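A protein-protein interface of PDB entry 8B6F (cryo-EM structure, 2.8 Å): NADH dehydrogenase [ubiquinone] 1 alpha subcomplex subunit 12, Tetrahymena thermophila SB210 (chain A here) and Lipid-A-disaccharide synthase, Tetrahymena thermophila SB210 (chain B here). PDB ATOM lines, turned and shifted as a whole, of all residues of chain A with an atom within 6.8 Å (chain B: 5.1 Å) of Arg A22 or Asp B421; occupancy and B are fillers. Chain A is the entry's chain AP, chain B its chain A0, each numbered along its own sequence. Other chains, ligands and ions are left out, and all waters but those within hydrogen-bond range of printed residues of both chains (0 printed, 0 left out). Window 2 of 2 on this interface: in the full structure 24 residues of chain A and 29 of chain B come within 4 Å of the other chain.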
ATOM      1  N   TRP A  17      12.234  13.871  -4.496  1.00  0.00           N
ATOM      2  CA  TRP A  17      11.606  14.995  -3.809  1.00  0.00           C
ATOM      3  C   TRP A  17      12.549  15.612  -2.785  1.00  0.00           C
ATOM      4  O   TRP A  17      12.620  16.841  -2.664  1.00  0.00           O
ATOM      5  CB  TRP A  17      10.303  14.538  -3.156  1.00  0.00           C
ATOM      6  CG  TRP A  17       9.315  14.033  -4.159  1.00  0.00           C
ATOM      7  CD1 TRP A  17       8.964  12.733  -4.380  1.00  0.00           C
ATOM      8  CD2 TRP A  17       8.563  14.817  -5.095  1.00  0.00           C
ATOM      9  NE1 TRP A  17       8.034  12.659  -5.389  1.00  0.00           N
ATOM     10  CE2 TRP A  17       7.770  13.925  -5.844  1.00  0.00           C
ATOM     11  CE3 TRP A  17       8.480  16.187  -5.367  1.00  0.00           C
ATOM     12  CZ2 TRP A  17       6.907  14.357  -6.850  1.00  0.00           C
ATOM     13  CZ3 TRP A  17       7.620  16.615  -6.366  1.00  0.00           C
ATOM     14  CH2 TRP A  17       6.845  15.703  -7.096  1.00  0.00           C
ATOM     15  N   VAL A  18      13.276  14.784  -2.036  1.00  0.00           N
ATOM     16  CA  VAL A  18      14.241  15.317  -1.079  1.00  0.00           C
ATOM     17  C   VAL A  18      15.335  16.085  -1.806  1.00  0.00           C
ATOM     18  O   VAL A  18      15.742  17.172  -1.379  1.00  0.00           O
ATOM     19  CB  VAL A  18      14.825  14.182  -0.217  1.00  0.00           C
ATOM     20  CG1 VAL A  18      15.882  14.722   0.738  1.00  0.00           C
ATOM     21  CG2 VAL A  18      13.720  13.486   0.558  1.00  0.00           C
ATOM     22  N   HIS A  19      15.838  15.529  -2.911  1.00  0.00           N
ATOM     23  CA  HIS A  19      16.885  16.206  -3.667  1.00  0.00           C
ATOM     24  C   HIS A  19      16.390  17.534  -4.225  1.00  0.00           C
ATOM     25  O   HIS A  19      17.107  18.540  -4.184  1.00  0.00           O
ATOM     26  CB  HIS A  19      17.383  15.302  -4.794  1.00  0.00           C
ATOM     27  CG  HIS A  19      18.765  15.631  -5.260  1.00  0.00           C
ATOM     28  ND1 HIS A  19      19.044  16.723  -6.054  1.00  0.00           N
ATOM     29  CD2 HIS A  19      19.950  15.015  -5.040  1.00  0.00           C
ATOM     30  CE1 HIS A  19      20.340  16.765  -6.302  1.00  0.00           C
ATOM     31  NE2 HIS A  19      20.913  15.740  -5.700  1.00  0.00           N
ATOM     32  N   LEU A  20      15.162  17.556  -4.746  1.00  0.00           N
ATOM     33  CA  LEU A  20      14.592  18.797  -5.256  1.00  0.00           C
ATOM     34  C   LEU A  20      14.433  19.823  -4.141  1.00  0.00           C
ATOM     35  O   LEU A  20      14.745  21.005  -4.323  1.00  0.00           O
ATOM     36  CB  LEU A  20      13.244  18.514  -5.922  1.00  0.00           C
ATOM     37  CG  LEU A  20      12.707  19.505  -6.964  1.00  0.00           C
ATOM     38  CD1 LEU A  20      11.374  19.018  -7.502  1.00  0.00           C
ATOM     39  CD2 LEU A  20      12.569  20.923  -6.431  1.00  0.00           C
ATOM     40  N   ARG A  21      13.977  19.384  -2.969  1.00  0.00           N
ATOM     41  CA  ARG A  21      13.783  20.310  -1.860  1.00  0.00           C
ATOM     42  C   ARG A  21      15.100  20.939  -1.425  1.00  0.00           C
ATOM     43  O   ARG A  21      15.158  22.145  -1.154  1.00  0.00           O
ATOM     44  CB  ARG A  21      13.127  19.584  -0.689  1.00  0.00           C
ATOM     45  CG  ARG A  21      12.686  20.494   0.444  1.00  0.00           C
ATOM     46  CD  ARG A  21      12.542  19.711   1.737  1.00  0.00           C
ATOM     47  NE  ARG A  21      11.753  18.499   1.552  1.00  0.00           N
ATOM     48  CZ  ARG A  21      11.611  17.550   2.465  1.00  0.00           C
ATOM     49  NH1 ARG A  21      12.196  17.635   3.648  1.00  0.00           N
ATOM     50  NH2 ARG A  21      10.864  16.485   2.184  1.00  0.00           N
ATOM     51  N   ARG A  22      16.168  20.148  -1.346  1.00  0.00           N
ATOM     52  CA  ARG A  22      17.431  20.637  -0.802  1.00  0.00           C
ATOM     53  C   ARG A  22      18.300  21.300  -1.870  1.00  0.00           C
ATOM     54  O   ARG A  22      18.620  22.487  -1.763  1.00  0.00           O
ATOM     55  CB  ARG A  22      18.188  19.487  -0.127  1.00  0.00           C
ATOM     56  CG  ARG A  22      19.593  19.862   0.314  1.00  0.00           C
ATOM     57  CD  ARG A  22      20.056  19.038   1.504  1.00  0.00           C
ATOM     58  NE  ARG A  22      19.730  19.690   2.769  1.00  0.00           N
ATOM     59  CZ  ARG A  22      18.645  19.446   3.494  1.00  0.00           C
ATOM     60  NH1 ARG A  22      17.749  18.547   3.123  1.00  0.00           N
ATOM     61  NH2 ARG A  22      18.455  20.123   4.622  1.00  0.00           N
ATOM     62  N   GLU A  23      18.686  20.551  -2.905  1.00  0.00           N
ATOM     63  CA  GLU A  23      19.618  21.093  -3.890  1.00  0.00           C
ATOM     64  C   GLU A  23      18.953  22.131  -4.787  1.00  0.00           C
ATOM     65  O   GLU A  23      19.530  23.192  -5.046  1.00  0.00           O
ATOM     66  CB  GLU A  23      20.212  19.964  -4.735  1.00  0.00           C
ATOM     67  CG  GLU A  23      21.446  19.319  -4.126  1.00  0.00           C
ATOM     68  CD  GLU A  23      21.157  18.633  -2.809  1.00  0.00           C
ATOM     69  OE1 GLU A  23      19.967  18.425  -2.498  1.00  0.00           O
ATOM     70  OE2 GLU A  23      22.119  18.304  -2.083  1.00  0.00           O
ATOM     71  N   GLY A  24      17.749  21.844  -5.275  1.00  0.00           N
ATOM     72  CA  GLY A  24      17.072  22.737  -6.197  1.00  0.00           C
ATOM     73  C   GLY A  24      16.786  22.074  -7.527  1.00  0.00           C
ATOM     74  O   GLY A  24      17.408  21.063  -7.863  1.00  0.00           O
ATOM     75  N   TYR A  50      19.091   9.741  -1.576  1.00  0.00           N
ATOM     76  CA  TYR A  50      20.159   9.880  -2.554  1.00  0.00           C
ATOM     77  C   TYR A  50      21.516   9.812  -1.868  1.00  0.00           C
ATOM     78  O   TYR A  50      21.678  10.243  -0.724  1.00  0.00           O
ATOM     79  CB  TYR A  50      20.029  11.190  -3.341  1.00  0.00           C
ATOM     80  CG  TYR A  50      20.178  12.448  -2.522  1.00  0.00           C
ATOM     81  CD1 TYR A  50      19.083  13.029  -1.901  1.00  0.00           C
ATOM     82  CD2 TYR A  50      21.410  13.072  -2.399  1.00  0.00           C
ATOM     83  CE1 TYR A  50      19.214  14.188  -1.163  1.00  0.00           C
ATOM     84  CE2 TYR A  50      21.553  14.231  -1.665  1.00  0.00           C
ATOM     85  CZ  TYR A  50      20.452  14.785  -1.051  1.00  0.00           C
ATOM     86  OH  TYR A  50      20.591  15.939  -0.317  1.00  0.00           O
ATOM     87  N   LYS B 295      19.262  23.526  12.996  1.00  0.00           N
ATOM     88  CA  LYS B 295      20.099  22.357  12.784  1.00  0.00           C
ATOM     89  C   LYS B 295      20.435  21.691  14.118  1.00  0.00           C
ATOM     90  O   LYS B 295      20.485  22.354  15.159  1.00  0.00           O
ATOM     91  CB  LYS B 295      21.390  22.739  12.062  1.00  0.00           C
ATOM     92  CG  LYS B 295      21.232  22.914  10.562  1.00  0.00           C
ATOM     93  CD  LYS B 295      22.574  23.185   9.904  1.00  0.00           C
ATOM     94  CE  LYS B 295      22.458  23.214   8.389  1.00  0.00           C
ATOM     95  NZ  LYS B 295      22.039  21.896   7.836  1.00  0.00           N
ATOM     96  N   THR B 412      17.783  28.229  -7.647  1.00  0.00           N
ATOM     97  CA  THR B 412      17.175  26.986  -7.192  1.00  0.00           C
ATOM     98  C   THR B 412      17.954  26.431  -6.012  1.00  0.00           C
ATOM     99  O   THR B 412      17.386  25.796  -5.119  1.00  0.00           O
ATOM    100  CB  THR B 412      17.108  25.958  -8.319  1.00  0.00           C
ATOM    101  OG1 THR B 412      18.393  25.840  -8.939  1.00  0.00           O
ATOM    102  CG2 THR B 412      16.073  26.369  -9.355  1.00  0.00           C
ATOM    103  N   ASN B 415      18.147  28.559  -1.812  1.00  0.00           N
ATOM    104  CA  ASN B 415      16.996  28.270  -0.979  1.00  0.00           C
ATOM    105  C   ASN B 415      17.439  28.111   0.468  1.00  0.00           C
ATOM    106  O   ASN B 415      18.624  27.890   0.742  1.00  0.00           O
ATOM    107  CB  ASN B 415      16.274  26.999  -1.452  1.00  0.00           C
ATOM    108  CG  ASN B 415      17.200  25.809  -1.564  1.00  0.00           C
ATOM    109  OD1 ASN B 415      17.454  25.111  -0.585  1.00  0.00           O
ATOM    110  ND2 ASN B 415      17.700  25.563  -2.767  1.00  0.00           N
ATOM    111  N   PRO B 416      16.514  28.228   1.423  1.00  0.00           N
ATOM    112  CA  PRO B 416      16.930  28.195   2.836  1.00  0.00           C
ATOM    113  C   PRO B 416      17.723  26.955   3.203  1.00  0.00           C
ATOM    114  O   PRO B 416      18.724  27.058   3.923  1.00  0.00           O
ATOM    115  CB  PRO B 416      15.595  28.261   3.591  1.00  0.00           C
ATOM    116  CG  PRO B 416      14.652  28.903   2.640  1.00  0.00           C
ATOM    117  CD  PRO B 416      15.065  28.441   1.279  1.00  0.00           C
ATOM    118  N   TYR B 417      17.306  25.781   2.732  1.00  0.00           N
ATOM    119  CA  TYR B 417      17.973  24.550   3.141  1.00  0.00           C
ATOM    120  C   TYR B 417      19.417  24.525   2.658  1.00  0.00           C
ATOM    121  O   TYR B 417      20.343  24.302   3.446  1.00  0.00           O
ATOM    122  CB  TYR B 417      17.210  23.341   2.602  1.00  0.00           C
ATOM    123  CG  TYR B 417      15.749  23.325   2.981  1.00  0.00           C
ATOM    124  CD1 TYR B 417      15.324  22.715   4.154  1.00  0.00           C
ATOM    125  CD2 TYR B 417      14.796  23.919   2.168  1.00  0.00           C
ATOM    126  CE1 TYR B 417      13.990  22.698   4.506  1.00  0.00           C
ATOM    127  CE2 TYR B 417      13.459  23.908   2.510  1.00  0.00           C
ATOM    128  CZ  TYR B 417      13.062  23.295   3.680  1.00  0.00           C
ATOM    129  OH  TYR B 417      11.731  23.281   4.025  1.00  0.00           O
ATOM    130  N   LYS B 418      19.629  24.748   1.360  1.00  0.00           N
ATOM    131  CA  LYS B 418      20.980  24.690   0.817  1.00  0.00           C
ATOM    132  C   LYS B 418      21.864  25.787   1.398  1.00  0.00           C
ATOM    133  O   LYS B 418      23.016  25.536   1.764  1.00  0.00           O
ATOM    134  CB  LYS B 418      20.929  24.795  -0.706  1.00  0.00           C
ATOM    135  CG  LYS B 418      22.245  24.486  -1.405  1.00  0.00           C
ATOM    136  CD  LYS B 418      22.628  23.021  -1.256  1.00  0.00           C
ATOM    137  CE  LYS B 418      23.857  22.678  -2.080  1.00  0.00           C
ATOM    138  NZ  LYS B 418      23.622  22.853  -3.539  1.00  0.00           N
ATOM    139  N   LEU B 419      21.335  27.008   1.508  1.00  0.00           N
ATOM    140  CA  LEU B 419      22.139  28.108   2.032  1.00  0.00           C
ATOM    141  C   LEU B 419      22.503  27.877   3.493  1.00  0.00           C
ATOM    142  O   LEU B 419      23.625  28.181   3.913  1.00  0.00           O
ATOM    143  CB  LEU B 419      21.418  29.444   1.836  1.00  0.00           C
ATOM    144  CG  LEU B 419      22.169  30.694   2.328  1.00  0.00           C
ATOM    145  CD1 LEU B 419      23.619  30.673   1.891  1.00  0.00           C
ATOM    146  CD2 LEU B 419      21.542  31.982   1.802  1.00  0.00           C
ATOM    147  N   SER B 420      21.570  27.343   4.285  1.00  0.00           N
ATOM    148  CA  SER B 420      21.890  27.017   5.670  1.00  0.00           C
ATOM    149  C   SER B 420      22.961  25.937   5.743  1.00  0.00           C
ATOM    150  O   SER B 420      23.867  26.006   6.581  1.00  0.00           O
ATOM    151  CB  SER B 420      20.630  26.571   6.414  1.00  0.00           C
ATOM    152  OG  SER B 420      20.100  25.382   5.855  1.00  0.00           O
ATOM    153  N   ASP B 421      22.877  24.927   4.874  1.00  0.00           N
ATOM    154  CA  ASP B 421      23.896  23.882   4.859  1.00  0.00           C
ATOM    155  C   ASP B 421      25.268  24.467   4.546  1.00  0.00           C
ATOM    156  O   ASP B 421      26.263  24.131   5.199  1.00  0.00           O
ATOM    157  CB  ASP B 421      23.531  22.801   3.841  1.00  0.00           C
ATOM    158  CG  ASP B 421      22.490  21.833   4.366  1.00  0.00           C
ATOM    159  OD1 ASP B 421      21.365  22.274   4.676  1.00  0.00           O
ATOM    160  OD2 ASP B 421      22.797  20.627   4.466  1.00  0.00           O
ATOM    161  N   GLU B 422      25.343  25.343   3.543  1.00  0.00           N
ATOM    162  CA  GLU B 422      26.628  25.927   3.174  1.00  0.00           C
ATOM    163  C   GLU B 422      27.158  26.832   4.280  1.00  0.00           C
ATOM    164  O   GLU B 422      28.358  26.820   4.577  1.00  0.00           O
ATOM    165  CB  GLU B 422      26.498  26.699   1.862  1.00  0.00           C
ATOM    166  CG  GLU B 422      26.031  25.851   0.687  1.00  0.00           C
ATOM    167  CD  GLU B 422      26.984  24.719   0.360  1.00  0.00           C
ATOM    168  OE1 GLU B 422      28.111  24.711   0.897  1.00  0.00           O
ATOM    169  OE2 GLU B 422      26.606  23.836  -0.438  1.00  0.00           O
ATOM    170  N   ILE B 423      26.284  27.630   4.894  1.00  0.00           N
ATOM    171  CA  ILE B 423      26.712  28.491   5.992  1.00  0.00           C
ATOM    172  C   ILE B 423      27.224  27.652   7.152  1.00  0.00           C
ATOM    173  O   ILE B 423      28.231  27.989   7.787  1.00  0.00           O
ATOM    174  CB  ILE B 423      25.563  29.422   6.427  1.00  0.00           C
ATOM    175  CG1 ILE B 423      25.280  30.452   5.333  1.00  0.00           C
ATOM    176  CG2 ILE B 423      25.901  30.127   7.740  1.00  0.00           C
ATOM    177  CD1 ILE B 423      24.034  31.281   5.572  1.00  0.00           C
ATOM    178  N   PHE B 424      26.545  26.542   7.448  1.00  0.00           N
ATOM    179  CA  PHE B 424      27.002  25.671   8.522  1.00  0.00           C
ATOM    180  C   PHE B 424      28.353  25.053   8.197  1.00  0.00           C
ATOM    181  O   PHE B 424      29.213  24.928   9.076  1.00  0.00           O
ATOM    182  CB  PHE B 424      25.970  24.578   8.794  1.00  0.00           C
ATOM    183  CG  PHE B 424      26.445  23.533   9.758  1.00  0.00           C
ATOM    184  CD1 PHE B 424      26.402  23.764  11.123  1.00  0.00           C
ATOM    185  CD2 PHE B 424      26.943  22.324   9.303  1.00  0.00           C
ATOM    186  CE1 PHE B 424      26.843  22.811  12.017  1.00  0.00           C
ATOM    187  CE2 PHE B 424      27.387  21.364  10.192  1.00  0.00           C
ATOM    188  CZ  PHE B 424      27.334  21.607  11.551  1.00  0.00           C
ATOM    189  N   ASP B 425      28.566  24.658   6.941  1.00  0.00           N
ATOM    190  CA  ASP B 425      29.861  24.104   6.565  1.00  0.00           C
ATOM    191  C   ASP B 425      30.969  25.125   6.789  1.00  0.00           C
ATOM    192  O   ASP B 425      32.020  24.805   7.355  1.00  0.00           O
ATOM    193  CB  ASP B 425      29.833  23.651   5.104  1.00  0.00           C
ATOM    194  CG  ASP B 425      28.708  22.674   4.817  1.00  0.00           C
ATOM    195  OD1 ASP B 425      28.219  22.030   5.767  1.00  0.00           O
ATOM    196  OD2 ASP B 425      28.311  22.550   3.639  1.00  0.00           O
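The backbone carbonyl oxygen (O) of Arg A22 lies close to the side-chain amide oxygen (OD1) of Asn B415, 3.1 Å away.
The guanidinium group (NE) of Arg A22 lies within salt-bridge range of the side-chain carboxylate (OD1) of Asp B421 (3.6 Å).
O of Glu A23 sits close to O of Thr B412, at 3.4 Å.
The side-chain amide oxygen (OD1) of Asn B415 sits close to the backbone NH (N) of Tyr B417 (3.4 Å).
OD1 of Asn B415 sits at hydrogen-bond distance from N of Lys B418, at 2.9 Å.
OD1 of Asp B421 lies close to O of Tyr B417, at 2.6 Å.
The side-chain carboxylate (OE2) of Glu A23 sits at hydrogen-bond distance from the side-chain hydroxyl (OH) of Tyr A50.
OD1 of Asp B421 is in salt-bridge range of NZ of Lys B295, 3.3 Å away.
The backbone carbonyl oxygen (O) of Tyr B417 lies within hydrogen-bond range of the side-chain hydroxyl (OG) of Ser B420, at 2.7 Å.
OD1 of Asn B415 touches O of Arg A21, at 3.8 Å.
Arg A21 touches Tyr B417 (O to CD2, 3.8 Å).
Arg A22 touches Tyr B417.
O of Arg A22 touches CB of Lys B418 (3.4 Å).
Glu A23 touches Asn B415.
O of Thr B412 touches CA of Gly A24, at 3.3 Å.
Of the printed residues of chain B, Arg A22 touches Asn B415 (3.1 Å), Tyr B417 (3.998 Å), Lys B418 (3.4 Å) and Asp B421 (3.6 Å).
Of the printed residues of chain B, Glu A23 touches Thr B412 and Asn B415.
Of the printed residues of chain A, Thr B412 touches Glu A23 and Gly A24.
Asp B421 touches just one residue of chain A: Arg A22.
Along chain A the printed residues that touch a printed residue of chain B span positions 21 to 24.
Printed residues of chain B that touch a printed residue of chain A: Thr B412, Asn B415, Tyr B417, Lys B418 and Asp B421.
Hydrophobic or aromatic side chains of chain B within 4 Å of the printed part of chain A: Tyr B417.
Among the printed residues, Asp or Glu carboxylates within 4 Å of a Lys or Arg side-chain nitrogen of the other chain: Arg A22 with Asp B421 (3.6 Å).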
